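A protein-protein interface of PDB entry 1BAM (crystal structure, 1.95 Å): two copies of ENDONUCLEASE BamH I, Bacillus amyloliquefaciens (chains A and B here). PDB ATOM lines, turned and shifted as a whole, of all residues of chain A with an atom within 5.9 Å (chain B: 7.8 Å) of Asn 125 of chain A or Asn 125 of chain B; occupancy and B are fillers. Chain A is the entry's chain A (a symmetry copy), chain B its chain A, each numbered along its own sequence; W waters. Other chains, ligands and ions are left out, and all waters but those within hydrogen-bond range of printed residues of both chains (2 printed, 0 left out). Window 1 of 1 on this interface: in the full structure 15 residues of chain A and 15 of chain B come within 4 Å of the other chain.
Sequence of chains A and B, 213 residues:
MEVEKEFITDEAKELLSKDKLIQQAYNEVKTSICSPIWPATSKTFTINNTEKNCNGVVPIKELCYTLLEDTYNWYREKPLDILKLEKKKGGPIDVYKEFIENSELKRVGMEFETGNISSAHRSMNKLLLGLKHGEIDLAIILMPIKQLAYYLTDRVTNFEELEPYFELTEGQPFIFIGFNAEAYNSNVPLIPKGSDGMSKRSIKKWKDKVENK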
ATOM      1  N   ALA A 120      17.766 -31.741   0.351  1.00  0.00           N
ATOM      2  CA  ALA A 120      18.953 -30.924   0.507  1.00  0.00           C
ATOM      3  C   ALA A 120      18.937 -30.203   1.850  1.00  0.00           C
ATOM      4  O   ALA A 120      19.972 -29.994   2.457  1.00  0.00           O
ATOM      5  CB  ALA A 120      19.060 -29.935  -0.657  1.00  0.00           C
ATOM      6  N   HIS A 121      17.759 -29.777   2.303  1.00  0.00           N
ATOM      7  CA  HIS A 121      17.655 -29.110   3.601  1.00  0.00           C
ATOM      8  C   HIS A 121      17.982 -30.060   4.707  1.00  0.00           C
ATOM      9  O   HIS A 121      18.707 -29.720   5.627  1.00  0.00           O
ATOM     10  CB  HIS A 121      16.253 -28.547   3.835  1.00  0.00           C
ATOM     11  CG  HIS A 121      16.036 -27.233   3.179  1.00  0.00           C
ATOM     12  ND1 HIS A 121      16.480 -26.053   3.742  1.00  0.00           N
ATOM     13  CD2 HIS A 121      15.466 -26.904   2.008  1.00  0.00           C
ATOM     14  CE1 HIS A 121      16.191 -25.056   2.924  1.00  0.00           C
ATOM     15  NE2 HIS A 121      15.575 -25.542   1.867  1.00  0.00           N
ATOM     16  N   ARG A 122      17.432 -31.255   4.621  1.00  0.00           N
ATOM     17  CA  ARG A 122      17.678 -32.272   5.622  1.00  0.00           C
ATOM     18  C   ARG A 122      19.173 -32.639   5.688  1.00  0.00           C
ATOM     19  O   ARG A 122      19.740 -32.812   6.761  1.00  0.00           O
ATOM     20  CB  ARG A 122      16.855 -33.499   5.278  1.00  0.00           C
ATOM     21  CG  ARG A 122      16.919 -34.536   6.332  1.00  0.00           C
ATOM     22  CD  ARG A 122      16.096 -35.694   5.902  1.00  0.00           C
ATOM     23  NE  ARG A 122      16.192 -36.774   6.868  1.00  0.00           N
ATOM     24  CZ  ARG A 122      15.724 -38.000   6.664  1.00  0.00           C
ATOM     25  NH1 ARG A 122      15.123 -38.309   5.522  1.00  0.00           N
ATOM     26  NH2 ARG A 122      15.845 -38.919   7.619  1.00  0.00           N
ATOM     27  N   SER A 123      19.807 -32.696   4.525  1.00  0.00           N
ATOM     28  CA  SER A 123      21.231 -33.026   4.410  1.00  0.00           C
ATOM     29  C   SER A 123      22.083 -31.938   5.031  1.00  0.00           C
ATOM     30  O   SER A 123      22.981 -32.224   5.817  1.00  0.00           O
ATOM     31  CB  SER A 123      21.585 -33.239   2.938  1.00  0.00           C
ATOM     32  OG  SER A 123      22.972 -33.424   2.764  1.00  0.00           O
ATOM     33  N   MET A 124      21.775 -30.683   4.709  1.00  0.00           N
ATOM     34  CA  MET A 124      22.506 -29.542   5.255  1.00  0.00           C
ATOM     35  C   MET A 124      22.403 -29.522   6.772  1.00  0.00           C
ATOM     36  O   MET A 124      23.394 -29.323   7.479  1.00  0.00           O
ATOM     37  CB  MET A 124      21.944 -28.239   4.683  1.00  0.00           C
ATOM     38  CG  MET A 124      22.582 -26.997   5.243  1.00  0.00           C
ATOM     39  SD  MET A 124      22.078 -25.559   4.357  1.00  0.00           S
ATOM     40  CE  MET A 124      20.556 -25.252   5.119  1.00  0.00           C
ATOM     41  N   ASN A 125      21.198 -29.732   7.285  1.00  0.00           N
ATOM     42  CA  ASN A 125      20.992 -29.724   8.731  1.00  0.00           C
ATOM     43  C   ASN A 125      21.696 -30.893   9.412  1.00  0.00           C
ATOM     44  O   ASN A 125      22.178 -30.767  10.537  1.00  0.00           O
ATOM     45  CB  ASN A 125      19.503 -29.726   9.057  1.00  0.00           C
ATOM     46  CG  ASN A 125      18.819 -28.411   8.711  1.00  0.00           C
ATOM     47  OD1 ASN A 125      17.584 -28.324   8.757  1.00  0.00           O
ATOM     48  ND2 ASN A 125      19.588 -27.392   8.379  1.00  0.00           N
ATOM     49  N   LYS A 126      21.717 -32.041   8.748  1.00  0.00           N
ATOM     50  CA  LYS A 126      22.390 -33.208   9.297  1.00  0.00           C
ATOM     51  C   LYS A 126      23.878 -32.887   9.526  1.00  0.00           C
ATOM     52  O   LYS A 126      24.424 -33.136  10.608  1.00  0.00           O
ATOM     53  CB  LYS A 126      22.201 -34.377   8.349  1.00  0.00           C
ATOM     54  CG  LYS A 126      22.879 -35.621   8.793  1.00  0.00           C
ATOM     55  CD  LYS A 126      22.459 -36.799   7.951  1.00  0.00           C
ATOM     56  CE  LYS A 126      23.182 -36.833   6.635  1.00  0.00           C
ATOM     57  NZ  LYS A 126      22.744 -38.024   5.835  1.00  0.00           N
ATOM     58  N   LEU A 127      24.496 -32.222   8.548  1.00  0.00           N
ATOM     59  CA  LEU A 127      25.900 -31.842   8.647  1.00  0.00           C
ATOM     60  C   LEU A 127      26.110 -30.739   9.660  1.00  0.00           C
ATOM     61  O   LEU A 127      27.090 -30.737  10.404  1.00  0.00           O
ATOM     62  CB  LEU A 127      26.449 -31.428   7.270  1.00  0.00           C
ATOM     63  CG  LEU A 127      26.502 -32.555   6.227  1.00  0.00           C
ATOM     64  CD1 LEU A 127      26.870 -32.024   4.871  1.00  0.00           C
ATOM     65  CD2 LEU A 127      27.482 -33.600   6.662  1.00  0.00           C
ATOM     66  N   LEU A 128      25.195 -29.786   9.682  1.00  0.00           N
ATOM     67  CA  LEU A 128      25.255 -28.684  10.628  1.00  0.00           C
ATOM     68  C   LEU A 128      25.219 -29.195  12.082  1.00  0.00           C
ATOM     69  O   LEU A 128      25.913 -28.672  12.959  1.00  0.00           O
ATOM     70  CB  LEU A 128      24.078 -27.761  10.356  1.00  0.00           C
ATOM     71  CG  LEU A 128      24.278 -26.249  10.335  1.00  0.00           C
ATOM     72  CD1 LEU A 128      25.595 -25.845   9.731  1.00  0.00           C
ATOM     73  CD2 LEU A 128      23.094 -25.641   9.571  1.00  0.00           C
ATOM     74  N   LEU A 129      24.417 -30.218  12.341  1.00  0.00           N
ATOM     75  CA  LEU A 129      24.338 -30.772  13.684  1.00  0.00           C
ATOM     76  C   LEU A 129      25.638 -31.569  13.983  1.00  0.00           C
ATOM     77  O   LEU A 129      26.144 -31.542  15.115  1.00  0.00           O
ATOM     78  CB  LEU A 129      23.104 -31.661  13.806  1.00  0.00           C
ATOM     79  CG  LEU A 129      22.736 -32.147  15.204  1.00  0.00           C
ATOM     80  CD1 LEU A 129      22.145 -31.002  16.015  1.00  0.00           C
ATOM     81  CD2 LEU A 129      21.728 -33.259  15.062  1.00  0.00           C
ATOM     82  N   GLY A 130      26.152 -32.297  12.987  1.00  0.00           N
ATOM     83  CA  GLY A 130      27.405 -33.029  13.163  1.00  0.00           C
ATOM     84  C   GLY A 130      28.511 -32.053  13.543  1.00  0.00           C
ATOM     85  O   GLY A 130      29.346 -32.361  14.392  1.00  0.00           O
ATOM     86  N   TYR A 165      19.719 -20.141   1.300  1.00  0.00           N
ATOM     87  CA  TYR A 165      19.935 -20.730   2.621  1.00  0.00           C
ATOM     88  C   TYR A 165      21.369 -21.014   3.061  1.00  0.00           C
ATOM     89  O   TYR A 165      21.576 -21.499   4.171  1.00  0.00           O
ATOM     90  CB  TYR A 165      19.132 -22.016   2.730  1.00  0.00           C
ATOM     91  CG  TYR A 165      17.662 -21.784   2.560  1.00  0.00           C
ATOM     92  CD1 TYR A 165      16.880 -21.382   3.649  1.00  0.00           C
ATOM     93  CD2 TYR A 165      17.049 -21.933   1.319  1.00  0.00           C
ATOM     94  CE1 TYR A 165      15.535 -21.142   3.509  1.00  0.00           C
ATOM     95  CE2 TYR A 165      15.699 -21.692   1.170  1.00  0.00           C
ATOM     96  CZ  TYR A 165      14.951 -21.295   2.278  1.00  0.00           C
ATOM     97  OH  TYR A 165      13.603 -21.063   2.163  1.00  0.00           O
ATOM     98  N   LEU A 168      22.507 -19.786   6.473  1.00  0.00           N
ATOM     99  CA  LEU A 168      22.216 -20.482   7.721  1.00  0.00           C
ATOM    100  C   LEU A 168      23.402 -21.247   8.271  1.00  0.00           C
ATOM    101  O   LEU A 168      23.390 -21.644   9.436  1.00  0.00           O
ATOM    102  CB  LEU A 168      21.038 -21.434   7.556  1.00  0.00           C
ATOM    103  CG  LEU A 168      19.700 -20.759   7.274  1.00  0.00           C
ATOM    104  CD1 LEU A 168      18.628 -21.795   7.335  1.00  0.00           C
ATOM    105  CD2 LEU A 168      19.428 -19.693   8.309  1.00  0.00           C
ATOM    106  N   ILE B 117       9.500 -35.745   7.123  1.00  0.00           N
ATOM    107  CA  ILE B 117      10.623 -35.160   7.839  1.00  0.00           C
ATOM    108  C   ILE B 117      11.472 -34.190   7.014  1.00  0.00           C
ATOM    109  O   ILE B 117      11.902 -33.168   7.532  1.00  0.00           O
ATOM    110  CB  ILE B 117      11.499 -36.253   8.500  1.00  0.00           C
ATOM    111  CG1 ILE B 117      12.552 -35.626   9.427  1.00  0.00           C
ATOM    112  CG2 ILE B 117      12.169 -37.101   7.430  1.00  0.00           C
ATOM    113  CD1 ILE B 117      11.976 -34.754  10.520  1.00  0.00           C
ATOM    114  N   SER B 118      11.716 -34.494   5.737  1.00  0.00           N
ATOM    115  CA  SER B 118      12.504 -33.597   4.880  1.00  0.00           C
ATOM    116  C   SER B 118      11.758 -32.274   4.750  1.00  0.00           C
ATOM    117  O   SER B 118      12.374 -31.209   4.788  1.00  0.00           O
ATOM    118  CB  SER B 118      12.765 -34.228   3.510  1.00  0.00           C
ATOM    119  OG  SER B 118      13.587 -35.372   3.678  1.00  0.00           O
ATOM    120  N   SER B 119      10.429 -32.353   4.634  1.00  0.00           N
ATOM    121  CA  SER B 119       9.546 -31.171   4.582  1.00  0.00           C
ATOM    122  C   SER B 119       9.721 -30.322   5.827  1.00  0.00           C
ATOM    123  O   SER B 119       9.748 -29.102   5.748  1.00  0.00           O
ATOM    124  CB  SER B 119       8.071 -31.583   4.590  1.00  0.00           C
ATOM    125  OG  SER B 119       7.614 -31.809   3.280  1.00  0.00           O
ATOM    126  N   ALA B 120       9.719 -30.980   6.979  1.00  0.00           N
ATOM    127  CA  ALA B 120       9.851 -30.302   8.253  1.00  0.00           C
ATOM    128  C   ALA B 120      11.172 -29.544   8.324  1.00  0.00           C
ATOM    129  O   ALA B 120      11.252 -28.489   8.926  1.00  0.00           O
ATOM    130  CB  ALA B 120       9.725 -31.312   9.396  1.00  0.00           C
ATOM    131  N   HIS B 121      12.231 -30.103   7.743  1.00  0.00           N
ATOM    132  CA  HIS B 121      13.525 -29.421   7.735  1.00  0.00           C
ATOM    133  C   HIS B 121      13.458 -28.177   6.910  1.00  0.00           C
ATOM    134  O   HIS B 121      13.951 -27.135   7.311  1.00  0.00           O
ATOM    135  CB  HIS B 121      14.633 -30.318   7.181  1.00  0.00           C
ATOM    136  CG  HIS B 121      15.175 -31.264   8.189  1.00  0.00           C
ATOM    137  ND1 HIS B 121      16.113 -30.876   9.125  1.00  0.00           N
ATOM    138  CD2 HIS B 121      14.897 -32.553   8.442  1.00  0.00           C
ATOM    139  CE1 HIS B 121      16.376 -31.902   9.915  1.00  0.00           C
ATOM    140  NE2 HIS B 121      15.656 -32.932   9.523  1.00  0.00           N
ATOM    141  N   ARG B 122      12.853 -28.291   5.744  1.00  0.00           N
ATOM    142  CA  ARG B 122      12.710 -27.157   4.855  1.00  0.00           C
ATOM    143  C   ARG B 122      11.880 -26.037   5.509  1.00  0.00           C
ATOM    144  O   ARG B 122      12.199 -24.858   5.397  1.00  0.00           O
ATOM    145  CB  ARG B 122      12.038 -27.626   3.577  1.00  0.00           C
ATOM    146  CG  ARG B 122      11.992 -26.569   2.544  1.00  0.00           C
ATOM    147  CD  ARG B 122      11.310 -27.116   1.343  1.00  0.00           C
ATOM    148  NE  ARG B 122      11.168 -26.089   0.326  1.00  0.00           N
ATOM    149  CZ  ARG B 122      10.434 -26.226  -0.773  1.00  0.00           C
ATOM    150  NH1 ARG B 122       9.770 -27.352  -1.003  1.00  0.00           N
ATOM    151  NH2 ARG B 122      10.379 -25.232  -1.656  1.00  0.00           N
ATOM    152  N   SER B 123      10.846 -26.433   6.240  1.00  0.00           N
ATOM    153  CA  SER B 123       9.957 -25.496   6.934  1.00  0.00           C
ATOM    154  C   SER B 123      10.699 -24.776   8.041  1.00  0.00           C
ATOM    155  O   SER B 123      10.625 -23.556   8.148  1.00  0.00           O
ATOM    156  CB  SER B 123       8.746 -26.255   7.477  1.00  0.00           C
ATOM    157  OG  SER B 123       7.930 -25.423   8.270  1.00  0.00           O
ATOM    158  N   MET B 124      11.450 -25.529   8.843  1.00  0.00           N
ATOM    159  CA  MET B 124      12.230 -24.956   9.936  1.00  0.00           C
ATOM    160  C   MET B 124      13.238 -23.951   9.398  1.00  0.00           C
ATOM    161  O   MET B 124      13.392 -22.850   9.935  1.00  0.00           O
ATOM    162  CB  MET B 124      12.963 -26.065  10.693  1.00  0.00           C
ATOM    163  CG  MET B 124      13.859 -25.569  11.795  1.00  0.00           C
ATOM    164  SD  MET B 124      14.459 -26.898  12.786  1.00  0.00           S
ATOM    165  CE  MET B 124      15.780 -27.432  11.806  1.00  0.00           C
ATOM    166  N   ASN B 125      13.930 -24.322   8.330  1.00  0.00           N
ATOM    167  CA  ASN B 125      14.928 -23.432   7.743  1.00  0.00           C
ATOM    168  C   ASN B 125      14.292 -22.186   7.135  1.00  0.00           C
ATOM    169  O   ASN B 125      14.875 -21.104   7.165  1.00  0.00           O
ATOM    170  CB  ASN B 125      15.760 -24.175   6.705  1.00  0.00           C
ATOM    171  CG  ASN B 125      16.694 -25.207   7.321  1.00  0.00           C
ATOM    172  OD1 ASN B 125      17.301 -26.007   6.594  1.00  0.00           O
ATOM    173  ND2 ASN B 125      16.829 -25.201   8.633  1.00  0.00           N
ATOM    174  N   LYS B 126      13.114 -22.350   6.546  1.00  0.00           N
ATOM    175  CA  LYS B 126      12.409 -21.219   5.962  1.00  0.00           C
ATOM    176  C   LYS B 126      12.135 -20.164   7.048  1.00  0.00           C
ATOM    177  O   LYS B 126      12.420 -18.973   6.867  1.00  0.00           O
ATOM    178  CB  LYS B 126      11.130 -21.716   5.317  1.00  0.00           C
ATOM    179  CG  LYS B 126      10.306 -20.636   4.716  1.00  0.00           C
ATOM    180  CD  LYS B 126       9.184 -21.208   3.886  1.00  0.00           C
ATOM    181  CE  LYS B 126       8.032 -21.659   4.738  1.00  0.00           C
ATOM    182  NZ  LYS B 126       6.935 -22.208   3.874  1.00  0.00           N
ATOM    183  N   LEU B 127      11.698 -20.624   8.222  1.00  0.00           N
ATOM    184  CA  LEU B 127      11.416 -19.732   9.340  1.00  0.00           C
ATOM    185  C   LEU B 127      12.684 -19.157   9.930  1.00  0.00           C
ATOM    186  O   LEU B 127      12.738 -17.987  10.306  1.00  0.00           O
ATOM    187  CB  LEU B 127      10.592 -20.456  10.420  1.00  0.00           C
ATOM    188  CG  LEU B 127       9.178 -20.873   9.987  1.00  0.00           C
ATOM    189  CD1 LEU B 127       8.521 -21.732  11.030  1.00  0.00           C
ATOM    190  CD2 LEU B 127       8.352 -19.653   9.719  1.00  0.00           C
ATOM    191  N   LEU B 128      13.709 -19.987  10.026  1.00  0.00           N
ATOM    192  CA  LEU B 128      14.998 -19.558  10.544  1.00  0.00           C
ATOM    193  C   LEU B 128      15.589 -18.417   9.691  1.00  0.00           C
ATOM    194  O   LEU B 128      16.188 -17.475  10.216  1.00  0.00           O
ATOM    195  CB  LEU B 128      15.929 -20.760  10.549  1.00  0.00           C
ATOM    196  CG  LEU B 128      16.823 -21.033  11.755  1.00  0.00           C
ATOM    197  CD1 LEU B 128      16.153 -20.702  13.060  1.00  0.00           C
ATOM    198  CD2 LEU B 128      17.242 -22.507  11.690  1.00  0.00           C
ATOM    199  N   LEU B 129      15.420 -18.497   8.379  1.00  0.00           N
ATOM    200  CA  LEU B 129      15.932 -17.452   7.505  1.00  0.00           C
ATOM    201  C   LEU B 129      15.047 -16.183   7.657  1.00  0.00           C
ATOM    202  O   LEU B 129      15.561 -15.054   7.630  1.00  0.00           O
ATOM    203  CB  LEU B 129      15.947 -17.945   6.061  1.00  0.00           C
ATOM    204  CG  LEU B 129      16.659 -17.069   5.037  1.00  0.00           C
ATOM    205  CD1 LEU B 129      18.167 -17.174   5.220  1.00  0.00           C
ATOM    206  CD2 LEU B 129      16.267 -17.544   3.661  1.00  0.00           C
ATOM    207  N   GLY B 130      13.729 -16.367   7.782  1.00  0.00           N
ATOM    208  CA  GLY B 130      12.831 -15.232   7.990  1.00  0.00           C
ATOM    209  C   GLY B 130      13.242 -14.488   9.254  1.00  0.00           C
ATOM    210  O   GLY B 130      13.221 -13.259   9.286  1.00  0.00           O
ATOM    211  N   LEU B 131      13.611 -15.226  10.300  1.00  0.00           N
ATOM    212  CA  LEU B 131      14.068 -14.652  11.569  1.00  0.00           C
ATOM    213  C   LEU B 131      15.381 -13.894  11.418  1.00  0.00           C
ATOM    214  O   LEU B 131      15.542 -12.786  11.952  1.00  0.00           O
ATOM    215  CB  LEU B 131      14.276 -15.756  12.609  1.00  0.00           C
ATOM    216  CG  LEU B 131      13.048 -16.300  13.368  1.00  0.00           C
ATOM    217  CD1 LEU B 131      13.354 -17.658  13.971  1.00  0.00           C
ATOM    218  CD2 LEU B 131      12.627 -15.338  14.466  1.00  0.00           C
ATOM    219  N   LYS B 132      16.348 -14.510  10.732  1.00  0.00           N
ATOM    220  CA  LYS B 132      17.650 -13.881  10.529  1.00  0.00           C
ATOM    221  C   LYS B 132      17.541 -12.567   9.769  1.00  0.00           C
ATOM    222  O   LYS B 132      18.250 -11.617  10.052  1.00  0.00           O
ATOM    223  CB  LYS B 132      18.588 -14.826   9.794  1.00  0.00           C
ATOM    224  CG  LYS B 132      19.206 -15.865  10.685  1.00  0.00           C
ATOM    225  CD  LYS B 132      20.377 -16.512   9.986  1.00  0.00           C
ATOM    226  CE  LYS B 132      21.344 -15.438   9.522  1.00  0.00           C
ATOM    227  NZ  LYS B 132      22.503 -15.984   8.766  1.00  0.00           N
ATOM    228  N   ILE B 141       6.443 -23.797  15.368  1.00  0.00           N
ATOM    229  CA  ILE B 141       6.094 -24.933  14.543  1.00  0.00           C
ATOM    230  C   ILE B 141       5.264 -25.908  15.370  1.00  0.00           C
ATOM    231  O   ILE B 141       5.564 -26.163  16.549  1.00  0.00           O
ATOM    232  CB  ILE B 141       7.336 -25.653  13.980  1.00  0.00           C
ATOM    233  CG1 ILE B 141       8.001 -24.785  12.924  1.00  0.00           C
ATOM    234  CG2 ILE B 141       6.937 -26.986  13.364  1.00  0.00           C
ATOM    235  CD1 ILE B 141       9.168 -25.445  12.234  1.00  0.00           C
ATOM    236  N   LEU B 162      11.886 -34.719  14.649  1.00  0.00           N
ATOM    237  CA  LEU B 162      12.582 -33.471  14.394  1.00  0.00           C
ATOM    238  C   LEU B 162      13.333 -33.005  15.621  1.00  0.00           C
ATOM    239  O   LEU B 162      14.262 -32.223  15.516  1.00  0.00           O
ATOM    240  CB  LEU B 162      11.624 -32.366  13.924  1.00  0.00           C
ATOM    241  CG  LEU B 162      12.325 -31.080  13.475  1.00  0.00           C
ATOM    242  CD1 LEU B 162      13.203 -31.407  12.279  1.00  0.00           C
ATOM    243  CD2 LEU B 162      11.324 -29.994  13.102  1.00  0.00           C
ATOM    244  N   PRO B 164      15.892 -33.985  17.596  1.00  0.00           N
ATOM    245  CA  PRO B 164      17.358 -33.868  17.669  1.00  0.00           C
ATOM    246  C   PRO B 164      17.877 -32.572  17.045  1.00  0.00           C
ATOM    247  O   PRO B 164      18.930 -32.061  17.433  1.00  0.00           O
ATOM    248  CB  PRO B 164      17.836 -35.084  16.870  1.00  0.00           C
ATOM    249  CG  PRO B 164      16.755 -36.084  17.082  1.00  0.00           C
ATOM    250  CD  PRO B 164      15.505 -35.239  16.923  1.00  0.00           C
ATOM    251  N   TYR B 165      17.090 -32.007  16.138  1.00  0.00           N
ATOM    252  CA  TYR B 165      17.441 -30.776  15.431  1.00  0.00           C
ATOM    253  C   TYR B 165      16.925 -29.450  15.986  1.00  0.00           C
ATOM    254  O   TYR B 165      17.215 -28.402  15.415  1.00  0.00           O
ATOM    255  CB  TYR B 165      17.005 -30.894  13.980  1.00  0.00           C
ATOM    256  CG  TYR B 165      17.672 -32.038  13.278  1.00  0.00           C
ATOM    257  CD1 TYR B 165      18.947 -31.880  12.723  1.00  0.00           C
ATOM    258  CD2 TYR B 165      17.054 -33.283  13.186  1.00  0.00           C
ATOM    259  CE1 TYR B 165      19.584 -32.922  12.097  1.00  0.00           C
ATOM    260  CE2 TYR B 165      17.689 -34.335  12.560  1.00  0.00           C
ATOM    261  CZ  TYR B 165      18.959 -34.141  12.017  1.00  0.00           C
ATOM    262  OH  TYR B 165      19.609 -35.165  11.374  1.00  0.00           O
ATOM    263  N   LEU B 168      19.386 -26.596  16.476  1.00  0.00           N
ATOM    264  CA  LEU B 168      19.835 -25.722  15.399  1.00  0.00           C
ATOM    265  C   LEU B 168      19.177 -24.358  15.422  1.00  0.00           C
ATOM    266  O   LEU B 168      19.652 -23.436  14.758  1.00  0.00           O
ATOM    267  CB  LEU B 168      19.605 -26.367  14.038  1.00  0.00           C
ATOM    268  CG  LEU B 168      20.435 -27.617  13.769  1.00  0.00           C
ATOM    269  CD1 LEU B 168      20.247 -28.010  12.343  1.00  0.00           C
ATOM    270  CD2 LEU B 168      21.897 -27.334  14.025  1.00  0.00           C
ATOM    271  N   THR B 169      18.094 -24.218  16.188  1.00  0.00           N
ATOM    272  CA  THR B 169      17.397 -22.942  16.278  1.00  0.00           C
ATOM    273  C   THR B 169      17.905 -22.084  17.419  1.00  0.00           C
ATOM    274  O   THR B 169      17.530 -20.929  17.531  1.00  0.00           O
ATOM    275  CB  THR B 169      15.890 -23.154  16.423  1.00  0.00           C
ATOM    276  OG1 THR B 169      15.636 -23.873  17.632  1.00  0.00           O
ATOM    277  CG2 THR B 169      15.347 -23.940  15.211  1.00  0.00           C
ATOM    278  N   PHE B 174      12.481 -19.311  18.901  1.00  0.00           N
ATOM    279  CA  PHE B 174      11.819 -20.394  18.187  1.00  0.00           C
ATOM    280  C   PHE B 174      11.095 -21.268  19.187  1.00  0.00           C
ATOM    281  O   PHE B 174      11.608 -21.524  20.278  1.00  0.00           O
ATOM    282  CB  PHE B 174      12.876 -21.233  17.423  1.00  0.00           C
ATOM    283  CG  PHE B 174      12.423 -21.723  16.052  1.00  0.00           C
ATOM    284  CD1 PHE B 174      11.437 -22.686  15.925  1.00  0.00           C
ATOM    285  CD2 PHE B 174      13.001 -21.222  14.895  1.00  0.00           C
ATOM    286  CE1 PHE B 174      11.039 -23.132  14.683  1.00  0.00           C
ATOM    287  CE2 PHE B 174      12.607 -21.669  13.654  1.00  0.00           C
ATOM    288  CZ  PHE B 174      11.626 -22.621  13.547  1.00  0.00           C
HETATM  289  O   HOH W   1      13.506 -24.221  -0.175  1.00  0.00           O
HETATM  290  O   HOH W   2      16.115 -36.078   9.821  1.00  0.00           O
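Printed residues of chain B within 4 Å of Arg 122 of chain A: Ile 117, Ser 118 and His 121.
Of the printed residues of chain B, Met 124 of chain A touches Asn 125 (3.7 Å).
Asn 125 of chain A touches five residues of chain B.
Of the printed residues of chain B, Tyr 165 of chain A touches Asn 125 (3.7 Å), Lys 126 (3.97 Å) and Leu 129 (3.7 Å).
Of the printed residues of chain B, Leu 168 of chain A touches Asn 125 (3.8 Å) and Lys 132 (3.7 Å).
Of the printed residues of chain A, Ser 118 of chain B touches Arg 122.
The nearest residue of chain B that does not touch Asn 125 of chain A is Arg 122 of chain B (5.6 Å).
The nearest residue of chain A that does not touch Asn 125 of chain B is Arg 122 of chain A (5.6 Å).
The nearest printed residue of chain A that does not touch Ser 118 of chain B is His 121 of chain A (4.8 Å).
Among the printed residues, merely in contact across the chains: Arg 122 of chain A with Ser 118 of chain B, His 121 of chain A with Arg 122 of chain B, Arg 122 of chain A with His 121 of chain B, Met 124 of chain A with Asn 125 of chain B, Asn 125 of chain A with Met 124 of chain B, Leu 129 of chain A with Pro 164 of chain B, Leu 129 of chain A with Tyr 165 of chain B, Tyr 165 of chain A with Leu 129 of chain B, Tyr 165 of chain A with Asn 125 of chain B, Asn 125 of chain A with Tyr 165 of chain B, Arg 122 of chain A with Ile 117 of chain B, Leu 168 of chain A with Lys 132 of chain B, Leu 168 of chain A with Asn 125 of chain B, Asn 125 of chain A with Leu 168 of chain B, Tyr 165 of chain A with Lys 126 of chain B and Lys 126 of chain A with Tyr 165 of chain B.
Printed residues of chain B that touch a printed residue of chain A: Ile 117, Ser 118, His 121, Arg 122, Met 124, Asn 125, Lys 126, Leu 129, Lys 132, Pro 164, Tyr 165 and Leu 168.
Hydrophobic or aromatic side chains of chain A that line the printed part of chain B: His 121, Met 124, Leu 129, Tyr 165 and Leu 168.
Among the printed residues, 19 pairs touch across the chains.
His 121 of chain A touches Arg 122 of chain B, and with the chains exchanged Arg 122 of chain A touches His 121 of chain B.
Met 124 of chain A touches Asn 125 of chain B, and with the chains exchanged Asn 125 of chain A touches Met 124 of chain B.
Asn 125 of chain A touches Tyr 165 of chain B, and with the chains exchanged Tyr 165 of chain A touches Asn 125 of chain B.
Asn 125 of chain A touches Leu 168 of chain B, and with the chains exchanged Leu 168 of chain A touches Asn 125 of chain B.
13 positions are printed for both chains.
Of the 19 pairs that touch across the chains among the printed residues, 15 have their exchanged pair printed and touching as well.
A ring nitrogen (ND1) of His 121 of chain B is in hydrogen-bond range of the side-chain amide oxygen (OD1) of Asn 125 of chain A, at 3.0 Å.
ND1 of His 121 of chain A sits at hydrogen-bond distance from OD1 of Asn 125 of chain B (3.0 Å).
The side-chain amide oxygen of Asn 125 of chain B sits close to the side-chain amide oxygen of Asn 125 of chain A (3.2 Å).
Water W1 bridges NE of Arg 122 of chain B (3.0 Å) and NE2 of His 121 of chain A (3.2 Å).
Water W2 bridges the guanidinium group of Arg 122 of chain A and a ring nitrogen (NE2) of His 121 of chain B.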
